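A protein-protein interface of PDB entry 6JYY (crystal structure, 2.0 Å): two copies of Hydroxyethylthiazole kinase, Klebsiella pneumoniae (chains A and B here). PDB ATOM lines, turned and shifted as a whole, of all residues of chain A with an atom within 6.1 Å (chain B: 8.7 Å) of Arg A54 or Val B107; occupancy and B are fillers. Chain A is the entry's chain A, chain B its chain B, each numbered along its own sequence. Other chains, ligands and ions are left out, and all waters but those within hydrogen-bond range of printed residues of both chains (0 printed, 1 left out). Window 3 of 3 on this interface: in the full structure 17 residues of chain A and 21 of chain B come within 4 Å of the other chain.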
ATOM      1  N   ILE A  51     -24.503 -12.171   8.159  1.00  0.00           N
ATOM      2  CA  ILE A  51     -25.965 -12.316   8.078  1.00  0.00           C
ATOM      3  C   ILE A  51     -26.818 -11.158   8.620  1.00  0.00           C
ATOM      4  O   ILE A  51     -27.998 -11.083   8.317  1.00  0.00           O
ATOM      5  CB  ILE A  51     -26.435 -13.629   8.793  1.00  0.00           C
ATOM      6  CG1 ILE A  51     -25.953 -13.708  10.247  1.00  0.00           C
ATOM      7  CG2 ILE A  51     -25.968 -14.838   8.002  1.00  0.00           C
ATOM      8  CD1 ILE A  51     -26.718 -14.740  11.105  1.00  0.00           C
ATOM      9  N   ASP A  52     -26.242 -10.263   9.405  1.00  0.00           N
ATOM     10  CA  ASP A  52     -26.960  -9.054   9.826  1.00  0.00           C
ATOM     11  C   ASP A  52     -27.251  -8.244   8.555  1.00  0.00           C
ATOM     12  O   ASP A  52     -26.401  -8.199   7.669  1.00  0.00           O
ATOM     13  CB  ASP A  52     -26.132  -8.251  10.837  1.00  0.00           C
ATOM     14  CG  ASP A  52     -26.663  -6.854  11.055  1.00  0.00           C
ATOM     15  OD1 ASP A  52     -27.523  -6.680  11.942  1.00  0.00           O
ATOM     16  OD2 ASP A  52     -26.225  -5.933  10.330  1.00  0.00           O
ATOM     17  N   PRO A  53     -28.456  -7.653   8.434  1.00  0.00           N
ATOM     18  CA  PRO A  53     -28.831  -7.019   7.157  1.00  0.00           C
ATOM     19  C   PRO A  53     -27.877  -5.887   6.750  1.00  0.00           C
ATOM     20  O   PRO A  53     -27.556  -5.694   5.560  1.00  0.00           O
ATOM     21  CB  PRO A  53     -30.238  -6.478   7.425  1.00  0.00           C
ATOM     22  CG  PRO A  53     -30.726  -7.188   8.583  1.00  0.00           C
ATOM     23  CD  PRO A  53     -29.556  -7.611   9.406  1.00  0.00           C
ATOM     24  N   ARG A  54     -27.376  -5.175   7.751  1.00  0.00           N
ATOM     25  CA  ARG A  54     -26.501  -4.040   7.505  1.00  0.00           C
ATOM     26  C   ARG A  54     -25.084  -4.491   7.241  1.00  0.00           C
ATOM     27  O   ARG A  54     -24.423  -3.991   6.317  1.00  0.00           O
ATOM     28  CB  ARG A  54     -26.547  -3.077   8.681  1.00  0.00           C
ATOM     29  CG  ARG A  54     -27.867  -2.322   8.793  1.00  0.00           C
ATOM     30  CD  ARG A  54     -27.886  -1.428  10.031  1.00  0.00           C
ATOM     31  NE  ARG A  54     -27.837  -2.224  11.254  1.00  0.00           N
ATOM     32  CZ  ARG A  54     -27.750  -1.727  12.485  1.00  0.00           C
ATOM     33  NH1 ARG A  54     -27.698  -0.418  12.681  1.00  0.00           N
ATOM     34  NH2 ARG A  54     -27.712  -2.551  13.527  1.00  0.00           N
ATOM     35  N   GLU A  55     -24.613  -5.456   8.025  1.00  0.00           N
ATOM     36  CA  GLU A  55     -23.289  -6.006   7.795  1.00  0.00           C
ATOM     37  C   GLU A  55     -23.250  -6.681   6.420  1.00  0.00           C
ATOM     38  O   GLU A  55     -22.238  -6.623   5.724  1.00  0.00           O
ATOM     39  CB  GLU A  55     -22.894  -7.019   8.865  1.00  0.00           C
ATOM     40  CG  GLU A  55     -22.614  -6.457  10.250  1.00  0.00           C
ATOM     41  CD  GLU A  55     -22.070  -7.533  11.218  1.00  0.00           C
ATOM     42  OE1 GLU A  55     -22.247  -8.744  10.946  1.00  0.00           O
ATOM     43  OE2 GLU A  55     -21.450  -7.169  12.242  1.00  0.00           O
ATOM     44  N   ALA A  56     -24.353  -7.327   6.045  1.00  0.00           N
ATOM     45  CA  ALA A  56     -24.375  -8.094   4.804  1.00  0.00           C
ATOM     46  C   ALA A  56     -24.408  -7.147   3.624  1.00  0.00           C
ATOM     47  O   ALA A  56     -23.712  -7.392   2.634  1.00  0.00           O
ATOM     48  CB  ALA A  56     -25.549  -9.041   4.757  1.00  0.00           C
ATOM     49  N   ALA A  57     -25.230  -6.092   3.714  1.00  0.00           N
ATOM     50  CA  ALA A  57     -25.133  -5.007   2.729  1.00  0.00           C
ATOM     51  C   ALA A  57     -23.693  -4.485   2.591  1.00  0.00           C
ATOM     52  O   ALA A  57     -23.178  -4.364   1.484  1.00  0.00           O
ATOM     53  CB  ALA A  57     -26.054  -3.869   3.097  1.00  0.00           C
ATOM     54  N   GLN A  58     -23.039  -4.158   3.705  1.00  0.00           N
ATOM     55  CA  GLN A  58     -21.662  -3.667   3.597  1.00  0.00           C
ATOM     56  C   GLN A  58     -20.711  -4.688   2.985  1.00  0.00           C
ATOM     57  O   GLN A  58     -19.819  -4.348   2.176  1.00  0.00           O
ATOM     58  CB  GLN A  58     -21.130  -3.256   4.966  1.00  0.00           C
ATOM     59  CG  GLN A  58     -19.609  -3.149   5.029  1.00  0.00           C
ATOM     60  CD  GLN A  58     -19.120  -2.432   6.278  1.00  0.00           C
ATOM     61  OE1 GLN A  58     -19.747  -2.500   7.345  1.00  0.00           O
ATOM     62  NE2 GLN A  58     -17.990  -1.735   6.152  1.00  0.00           N
ATOM     63  N   PHE A  59     -20.867  -5.945   3.387  1.00  0.00           N
ATOM     64  CA  PHE A  59     -19.877  -6.932   3.014  1.00  0.00           C
ATOM     65  C   PHE A  59     -20.057  -7.400   1.580  1.00  0.00           C
ATOM     66  O   PHE A  59     -19.074  -7.707   0.908  1.00  0.00           O
ATOM     67  CB  PHE A  59     -19.910  -8.129   3.959  1.00  0.00           C
ATOM     68  CG  PHE A  59     -18.741  -9.029   3.777  1.00  0.00           C
ATOM     69  CD1 PHE A  59     -17.488  -8.629   4.185  1.00  0.00           C
ATOM     70  CD2 PHE A  59     -18.876 -10.242   3.152  1.00  0.00           C
ATOM     71  CE1 PHE A  59     -16.399  -9.434   4.007  1.00  0.00           C
ATOM     72  CE2 PHE A  59     -17.785 -11.041   2.958  1.00  0.00           C
ATOM     73  CZ  PHE A  59     -16.550 -10.639   3.383  1.00  0.00           C
ATOM     74  N   VAL B  70     -18.553 -12.903  18.233  1.00  0.00           N
ATOM     75  CA  VAL B  70     -19.499 -12.094  17.440  1.00  0.00           C
ATOM     76  C   VAL B  70     -19.486 -12.367  15.922  1.00  0.00           C
ATOM     77  O   VAL B  70     -20.015 -11.580  15.109  1.00  0.00           O
ATOM     78  CB  VAL B  70     -19.226 -10.579  17.650  1.00  0.00           C
ATOM     79  CG1 VAL B  70     -19.523 -10.165  19.079  1.00  0.00           C
ATOM     80  CG2 VAL B  70     -17.805 -10.214  17.255  1.00  0.00           C
ATOM     81  N   LEU B  73     -22.932 -12.123  14.071  1.00  0.00           N
ATOM     82  CA  LEU B  73     -23.770 -11.327  14.956  1.00  0.00           C
ATOM     83  C   LEU B  73     -25.089 -10.966  14.292  1.00  0.00           C
ATOM     84  O   LEU B  73     -25.135 -10.719  13.104  1.00  0.00           O
ATOM     85  CB  LEU B  73     -23.027 -10.061  15.383  1.00  0.00           C
ATOM     86  CG  LEU B  73     -23.677  -9.279  16.533  1.00  0.00           C
ATOM     87  CD1 LEU B  73     -23.494 -10.023  17.843  1.00  0.00           C
ATOM     88  CD2 LEU B  73     -23.119  -7.877  16.634  1.00  0.00           C
ATOM     89  N   THR B  74     -26.163 -10.994  15.068  1.00  0.00           N
ATOM     90  CA  THR B  74     -27.450 -10.462  14.661  1.00  0.00           C
ATOM     91  C   THR B  74     -28.000  -9.639  15.806  1.00  0.00           C
ATOM     92  O   THR B  74     -27.501  -9.708  16.919  1.00  0.00           O
ATOM     93  CB  THR B  74     -28.485 -11.559  14.293  1.00  0.00           C
ATOM     94  OG1 THR B  74     -28.693 -12.428  15.414  1.00  0.00           O
ATOM     95  CG2 THR B  74     -28.028 -12.378  13.079  1.00  0.00           C
ATOM     96  N   GLU B  75     -29.042  -8.872  15.520  1.00  0.00           N
ATOM     97  CA  GLU B  75     -29.625  -7.950  16.478  1.00  0.00           C
ATOM     98  C   GLU B  75     -30.200  -8.709  17.669  1.00  0.00           C
ATOM     99  O   GLU B  75     -29.923  -8.370  18.813  1.00  0.00           O
ATOM    100  CB  GLU B  75     -30.706  -7.092  15.797  1.00  0.00           C
ATOM    101  CG  GLU B  75     -31.559  -7.830  14.735  1.00  0.00           C
ATOM    102  CD  GLU B  75     -30.978  -7.763  13.298  1.00  0.00           C
ATOM    103  OE1 GLU B  75     -30.044  -8.555  12.972  1.00  0.00           O
ATOM    104  OE2 GLU B  75     -31.470  -6.925  12.497  1.00  0.00           O
ATOM    105  N   ALA B  78     -27.488 -10.284  19.844  1.00  0.00           N
ATOM    106  CA  ALA B  78     -26.796  -9.264  20.609  1.00  0.00           C
ATOM    107  C   ALA B  78     -27.525  -8.972  21.939  1.00  0.00           C
ATOM    108  O   ALA B  78     -26.883  -8.836  22.991  1.00  0.00           O
ATOM    109  CB  ALA B  78     -26.648  -7.999  19.767  1.00  0.00           C
ATOM    110  N   VAL B 100     -14.352 -11.274  16.421  1.00  0.00           N
ATOM    111  CA  VAL B 100     -14.258 -11.643  15.011  1.00  0.00           C
ATOM    112  C   VAL B 100     -14.629 -10.481  14.072  1.00  0.00           C
ATOM    113  O   VAL B 100     -15.753  -9.950  14.117  1.00  0.00           O
ATOM    114  CB  VAL B 100     -15.178 -12.866  14.689  1.00  0.00           C
ATOM    115  CG1 VAL B 100     -15.069 -13.281  13.203  1.00  0.00           C
ATOM    116  CG2 VAL B 100     -14.791 -14.038  15.537  1.00  0.00           C
ATOM    117  N   ALA B 101     -13.662 -10.078  13.242  1.00  0.00           N
ATOM    118  CA  ALA B 101     -13.901  -9.146  12.140  1.00  0.00           C
ATOM    119  C   ALA B 101     -14.248  -7.725  12.596  1.00  0.00           C
ATOM    120  O   ALA B 101     -14.856  -6.952  11.855  1.00  0.00           O
ATOM    121  CB  ALA B 101     -15.010  -9.691  11.224  1.00  0.00           C
ATOM    122  N   VAL B 102     -13.840  -7.376  13.814  1.00  0.00           N
ATOM    123  CA  VAL B 102     -13.979  -6.005  14.310  1.00  0.00           C
ATOM    124  C   VAL B 102     -13.047  -5.078  13.537  1.00  0.00           C
ATOM    125  O   VAL B 102     -11.909  -5.434  13.242  1.00  0.00           O
ATOM    126  CB  VAL B 102     -13.684  -5.924  15.820  1.00  0.00           C
ATOM    127  CG1 VAL B 102     -13.366  -4.494  16.259  1.00  0.00           C
ATOM    128  CG2 VAL B 102     -14.876  -6.462  16.597  1.00  0.00           C
ATOM    129  N   GLY B 103     -13.547  -3.891  13.219  1.00  0.00           N
ATOM    130  CA  GLY B 103     -12.844  -2.961  12.353  1.00  0.00           C
ATOM    131  C   GLY B 103     -13.402  -3.065  10.945  1.00  0.00           C
ATOM    132  O   GLY B 103     -13.706  -2.053  10.300  1.00  0.00           O
ATOM    133  N   ALA B 104     -13.581  -4.306  10.492  1.00  0.00           N
ATOM    134  CA  ALA B 104     -13.929  -4.592   9.104  1.00  0.00           C
ATOM    135  C   ALA B 104     -15.437  -4.615   8.870  1.00  0.00           C
ATOM    136  O   ALA B 104     -15.890  -4.562   7.723  1.00  0.00           O
ATOM    137  CB  ALA B 104     -13.314  -5.914   8.684  1.00  0.00           C
ATOM    138  N   LEU B 105     -16.211  -4.697   9.948  1.00  0.00           N
ATOM    139  CA  LEU B 105     -17.668  -4.610   9.855  1.00  0.00           C
ATOM    140  C   LEU B 105     -18.185  -3.723  10.980  1.00  0.00           C
ATOM    141  O   LEU B 105     -17.860  -3.945  12.137  1.00  0.00           O
ATOM    142  CB  LEU B 105     -18.306  -6.007   9.922  1.00  0.00           C
ATOM    143  CG  LEU B 105     -17.900  -7.012   8.830  1.00  0.00           C
ATOM    144  CD1 LEU B 105     -18.284  -8.408   9.240  1.00  0.00           C
ATOM    145  CD2 LEU B 105     -18.555  -6.680   7.528  1.00  0.00           C
ATOM    146  N   THR B 106     -19.003  -2.734  10.630  1.00  0.00           N
ATOM    147  CA  THR B 106     -19.415  -1.676  11.554  1.00  0.00           C
ATOM    148  C   THR B 106     -20.248  -2.129  12.773  1.00  0.00           C
ATOM    149  O   THR B 106     -19.878  -1.849  13.929  1.00  0.00           O
ATOM    150  CB  THR B 106     -20.226  -0.604  10.785  1.00  0.00           C
ATOM    151  OG1 THR B 106     -19.395  -0.021   9.773  1.00  0.00           O
ATOM    152  CG2 THR B 106     -20.741   0.502  11.726  1.00  0.00           C
ATOM    153  N   VAL B 107     -21.364  -2.808  12.505  1.00  0.00           N
ATOM    154  CA  VAL B 107     -22.365  -3.112  13.531  1.00  0.00           C
ATOM    155  C   VAL B 107     -21.753  -3.830  14.743  1.00  0.00           C
ATOM    156  O   VAL B 107     -21.970  -3.435  15.913  1.00  0.00           O
ATOM    157  CB  VAL B 107     -23.503  -3.973  12.947  1.00  0.00           C
ATOM    158  CG1 VAL B 107     -24.539  -4.317  14.028  1.00  0.00           C
ATOM    159  CG2 VAL B 107     -24.175  -3.243  11.783  1.00  0.00           C
ATOM    160  N   ARG B 108     -20.971  -4.869  14.452  1.00  0.00           N
ATOM    161  CA  ARG B 108     -20.334  -5.656  15.492  1.00  0.00           C
ATOM    162  C   ARG B 108     -19.170  -4.887  16.133  1.00  0.00           C
ATOM    163  O   ARG B 108     -18.834  -5.128  17.298  1.00  0.00           O
ATOM    164  CB  ARG B 108     -19.857  -6.997  14.930  1.00  0.00           C
ATOM    165  CG  ARG B 108     -18.769  -6.908  13.891  1.00  0.00           C
ATOM    166  CD  ARG B 108     -18.402  -8.287  13.401  1.00  0.00           C
ATOM    167  NE  ARG B 108     -19.497  -8.906  12.647  1.00  0.00           N
ATOM    168  CZ  ARG B 108     -19.418 -10.091  12.047  1.00  0.00           C
ATOM    169  NH1 ARG B 108     -18.300 -10.806  12.118  1.00  0.00           N
ATOM    170  NH2 ARG B 108     -20.462 -10.572  11.373  1.00  0.00           N
ATOM    171  N   THR B 109     -18.570  -3.954  15.395  1.00  0.00           N
ATOM    172  CA  THR B 109     -17.469  -3.155  15.951  1.00  0.00           C
ATOM    173  C   THR B 109     -18.052  -2.262  17.076  1.00  0.00           C
ATOM    174  O   THR B 109     -17.546  -2.216  18.228  1.00  0.00           O
ATOM    175  CB  THR B 109     -16.750  -2.307  14.834  1.00  0.00           C
ATOM    176  OG1 THR B 109     -16.193  -3.174  13.840  1.00  0.00           O
ATOM    177  CG2 THR B 109     -15.616  -1.459  15.406  1.00  0.00           C
ATOM    178  N   ALA B 110     -19.165  -1.609  16.758  1.00  0.00           N
ATOM    179  CA  ALA B 110     -19.868  -0.814  17.766  1.00  0.00           C
ATOM    180  C   ALA B 110     -20.303  -1.672  18.971  1.00  0.00           C
ATOM    181  O   ALA B 110     -20.076  -1.305  20.139  1.00  0.00           O
ATOM    182  CB  ALA B 110     -21.080  -0.112  17.134  1.00  0.00           C
ATOM    183  N   PHE B 111     -20.932  -2.815  18.688  1.00  0.00           N
ATOM    184  CA  PHE B 111     -21.334  -3.729  19.761  1.00  0.00           C
ATOM    185  C   PHE B 111     -20.180  -4.154  20.695  1.00  0.00           C
ATOM    186  O   PHE B 111     -20.326  -4.169  21.946  1.00  0.00           O
ATOM    187  CB  PHE B 111     -22.005  -4.965  19.138  1.00  0.00           C
ATOM    188  CG  PHE B 111     -22.427  -6.002  20.133  1.00  0.00           C
ATOM    189  CD1 PHE B 111     -23.442  -5.746  21.039  1.00  0.00           C
ATOM    190  CD2 PHE B 111     -21.813  -7.245  20.154  1.00  0.00           C
ATOM    191  CE1 PHE B 111     -23.829  -6.716  21.954  1.00  0.00           C
ATOM    192  CE2 PHE B 111     -22.198  -8.203  21.062  1.00  0.00           C
ATOM    193  CZ  PHE B 111     -23.205  -7.936  21.964  1.00  0.00           C
ATOM    194  N   CYS B 112     -19.041  -4.509  20.105  1.00  0.00           N
ATOM    195  CA  CYS B 112     -17.873  -4.868  20.892  1.00  0.00           C
ATOM    196  C   CYS B 112     -17.452  -3.722  21.822  1.00  0.00           C
ATOM    197  O   CYS B 112     -17.250  -3.926  23.036  1.00  0.00           O
ATOM    198  CB  CYS B 112     -16.715  -5.266  19.984  1.00  0.00           C
ATOM    199  SG  CYS B 112     -16.930  -6.915  19.215  1.00  0.00           S
ATOM    200  N   HIS B 113     -17.328  -2.518  21.269  1.00  0.00           N
ATOM    201  CA  HIS B 113     -17.035  -1.379  22.142  1.00  0.00           C
ATOM    202  C   HIS B 113     -18.081  -1.219  23.258  1.00  0.00           C
ATOM    203  O   HIS B 113     -17.717  -0.894  24.386  1.00  0.00           O
ATOM    204  CB  HIS B 113     -16.923  -0.092  21.335  1.00  0.00           C
ATOM    205  CG  HIS B 113     -15.729  -0.051  20.434  1.00  0.00           C
ATOM    206  ND1 HIS B 113     -15.795   0.390  19.129  1.00  0.00           N
ATOM    207  CD2 HIS B 113     -14.437  -0.398  20.647  1.00  0.00           C
ATOM    208  CE1 HIS B 113     -14.598   0.312  18.577  1.00  0.00           C
ATOM    209  NE2 HIS B 113     -13.757  -0.170  19.473  1.00  0.00           N
ATOM    210  N   GLU B 114     -19.369  -1.441  22.982  1.00  0.00           N
ATOM    211  CA  GLU B 114     -20.340  -1.452  24.097  1.00  0.00           C
ATOM    212  C   GLU B 114     -19.972  -2.463  25.177  1.00  0.00           C
ATOM    213  O   GLU B 114     -20.038  -2.154  26.367  1.00  0.00           O
ATOM    214  CB  GLU B 114     -21.758  -1.783  23.638  1.00  0.00           C
ATOM    215  CG  GLU B 114     -22.326  -0.871  22.596  1.00  0.00           C
ATOM    216  CD  GLU B 114     -23.657  -1.374  22.071  1.00  0.00           C
ATOM    217  OE1 GLU B 114     -24.325  -2.159  22.794  1.00  0.00           O
ATOM    218  OE2 GLU B 114     -24.023  -0.995  20.931  1.00  0.00           O
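No position is printed for both chains.
Of chain B, only Val B107 (3.7 Å) comes within 4 Å of Arg A54. Val B107 touches just these residues of chain A: Asp A52, Arg A54 and Glu A55. Pro A53 touches one residue of chain B. Printed residues of chain B within 4 Å of Gln A58: Ala B104 (3.9 Å), Leu B105 (3.9 Å) and Thr B106 (3.4 Å). Of the printed residues of chain A, Leu B105 touches Gln A58 (3.9 Å). Of the printed residues of chain B, Glu A55 touches Val B107 and Arg B108. Printed residues of chain A within 4 Å of Thr B74: Ile A51. Ala A57 touches none of the printed residues of chain B. The nearest residue of chain B that does not touch Arg A54 is Glu B75 (5.9 Å).
The guanidinium group (NH2) of Arg B108 lies within salt-bridge range of the side-chain carboxylate (OE1) of Glu A55, at 2.6 Å. The side-chain carboxylate of Glu B75 lies close to the side-chain carboxylate of Asp A52 (3.3 Å). The backbone NH (N) of Thr B106 sits at hydrogen-bond distance from the side-chain amide oxygen (OE1) of Gln A58, at 3.4 Å.
Among the printed residues, merely in contact across the chains: Ile A51 with Thr B74 (3.3 Å), Asp A52 with Leu B73 (3.5 Å), Asp A52 with Val B107 (3.7 Å), Pro A53 with Glu B75 (3.7 Å), Arg A54 with Val B107 (3.7 Å), Glu A55 with Val B107 (3.8 Å), Gln A58 with Ala B104 (3.9 Å) and Gln A58 with Leu B105 (3.9 Å).
The side-chain carboxylate (OD2) of Asp A52 is in hydrogen-bond range of the backbone NH (N) of Arg A54 (2.9 Å). The side-chain carboxylate of Asp A52 is in hydrogen-bond range of the backbone NH of Glu A55 (2.9 Å). SG of Cys B112 lies within hydrogen-bond range of O of Arg B108 (3.2 Å). O of Leu B105 sits at hydrogen-bond distance from OG1 of Thr B109 (2.5 Å). The guanidinium group (NH1) of Arg B108 sits close to the backbone carbonyl oxygen (O) of Val B100 (3.3 Å).
Of the 9 printed residues of chain A, 6 touch a printed residue of chain B. Hydrophobic or aromatic side chains of chain A that line the printed part of chain B: Ile A51 and Pro A53. Among the printed residues, Asp or Glu carboxylates within 4 Å of a Lys or Arg side-chain nitrogen of the other chain: Glu A55 with Arg B108.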
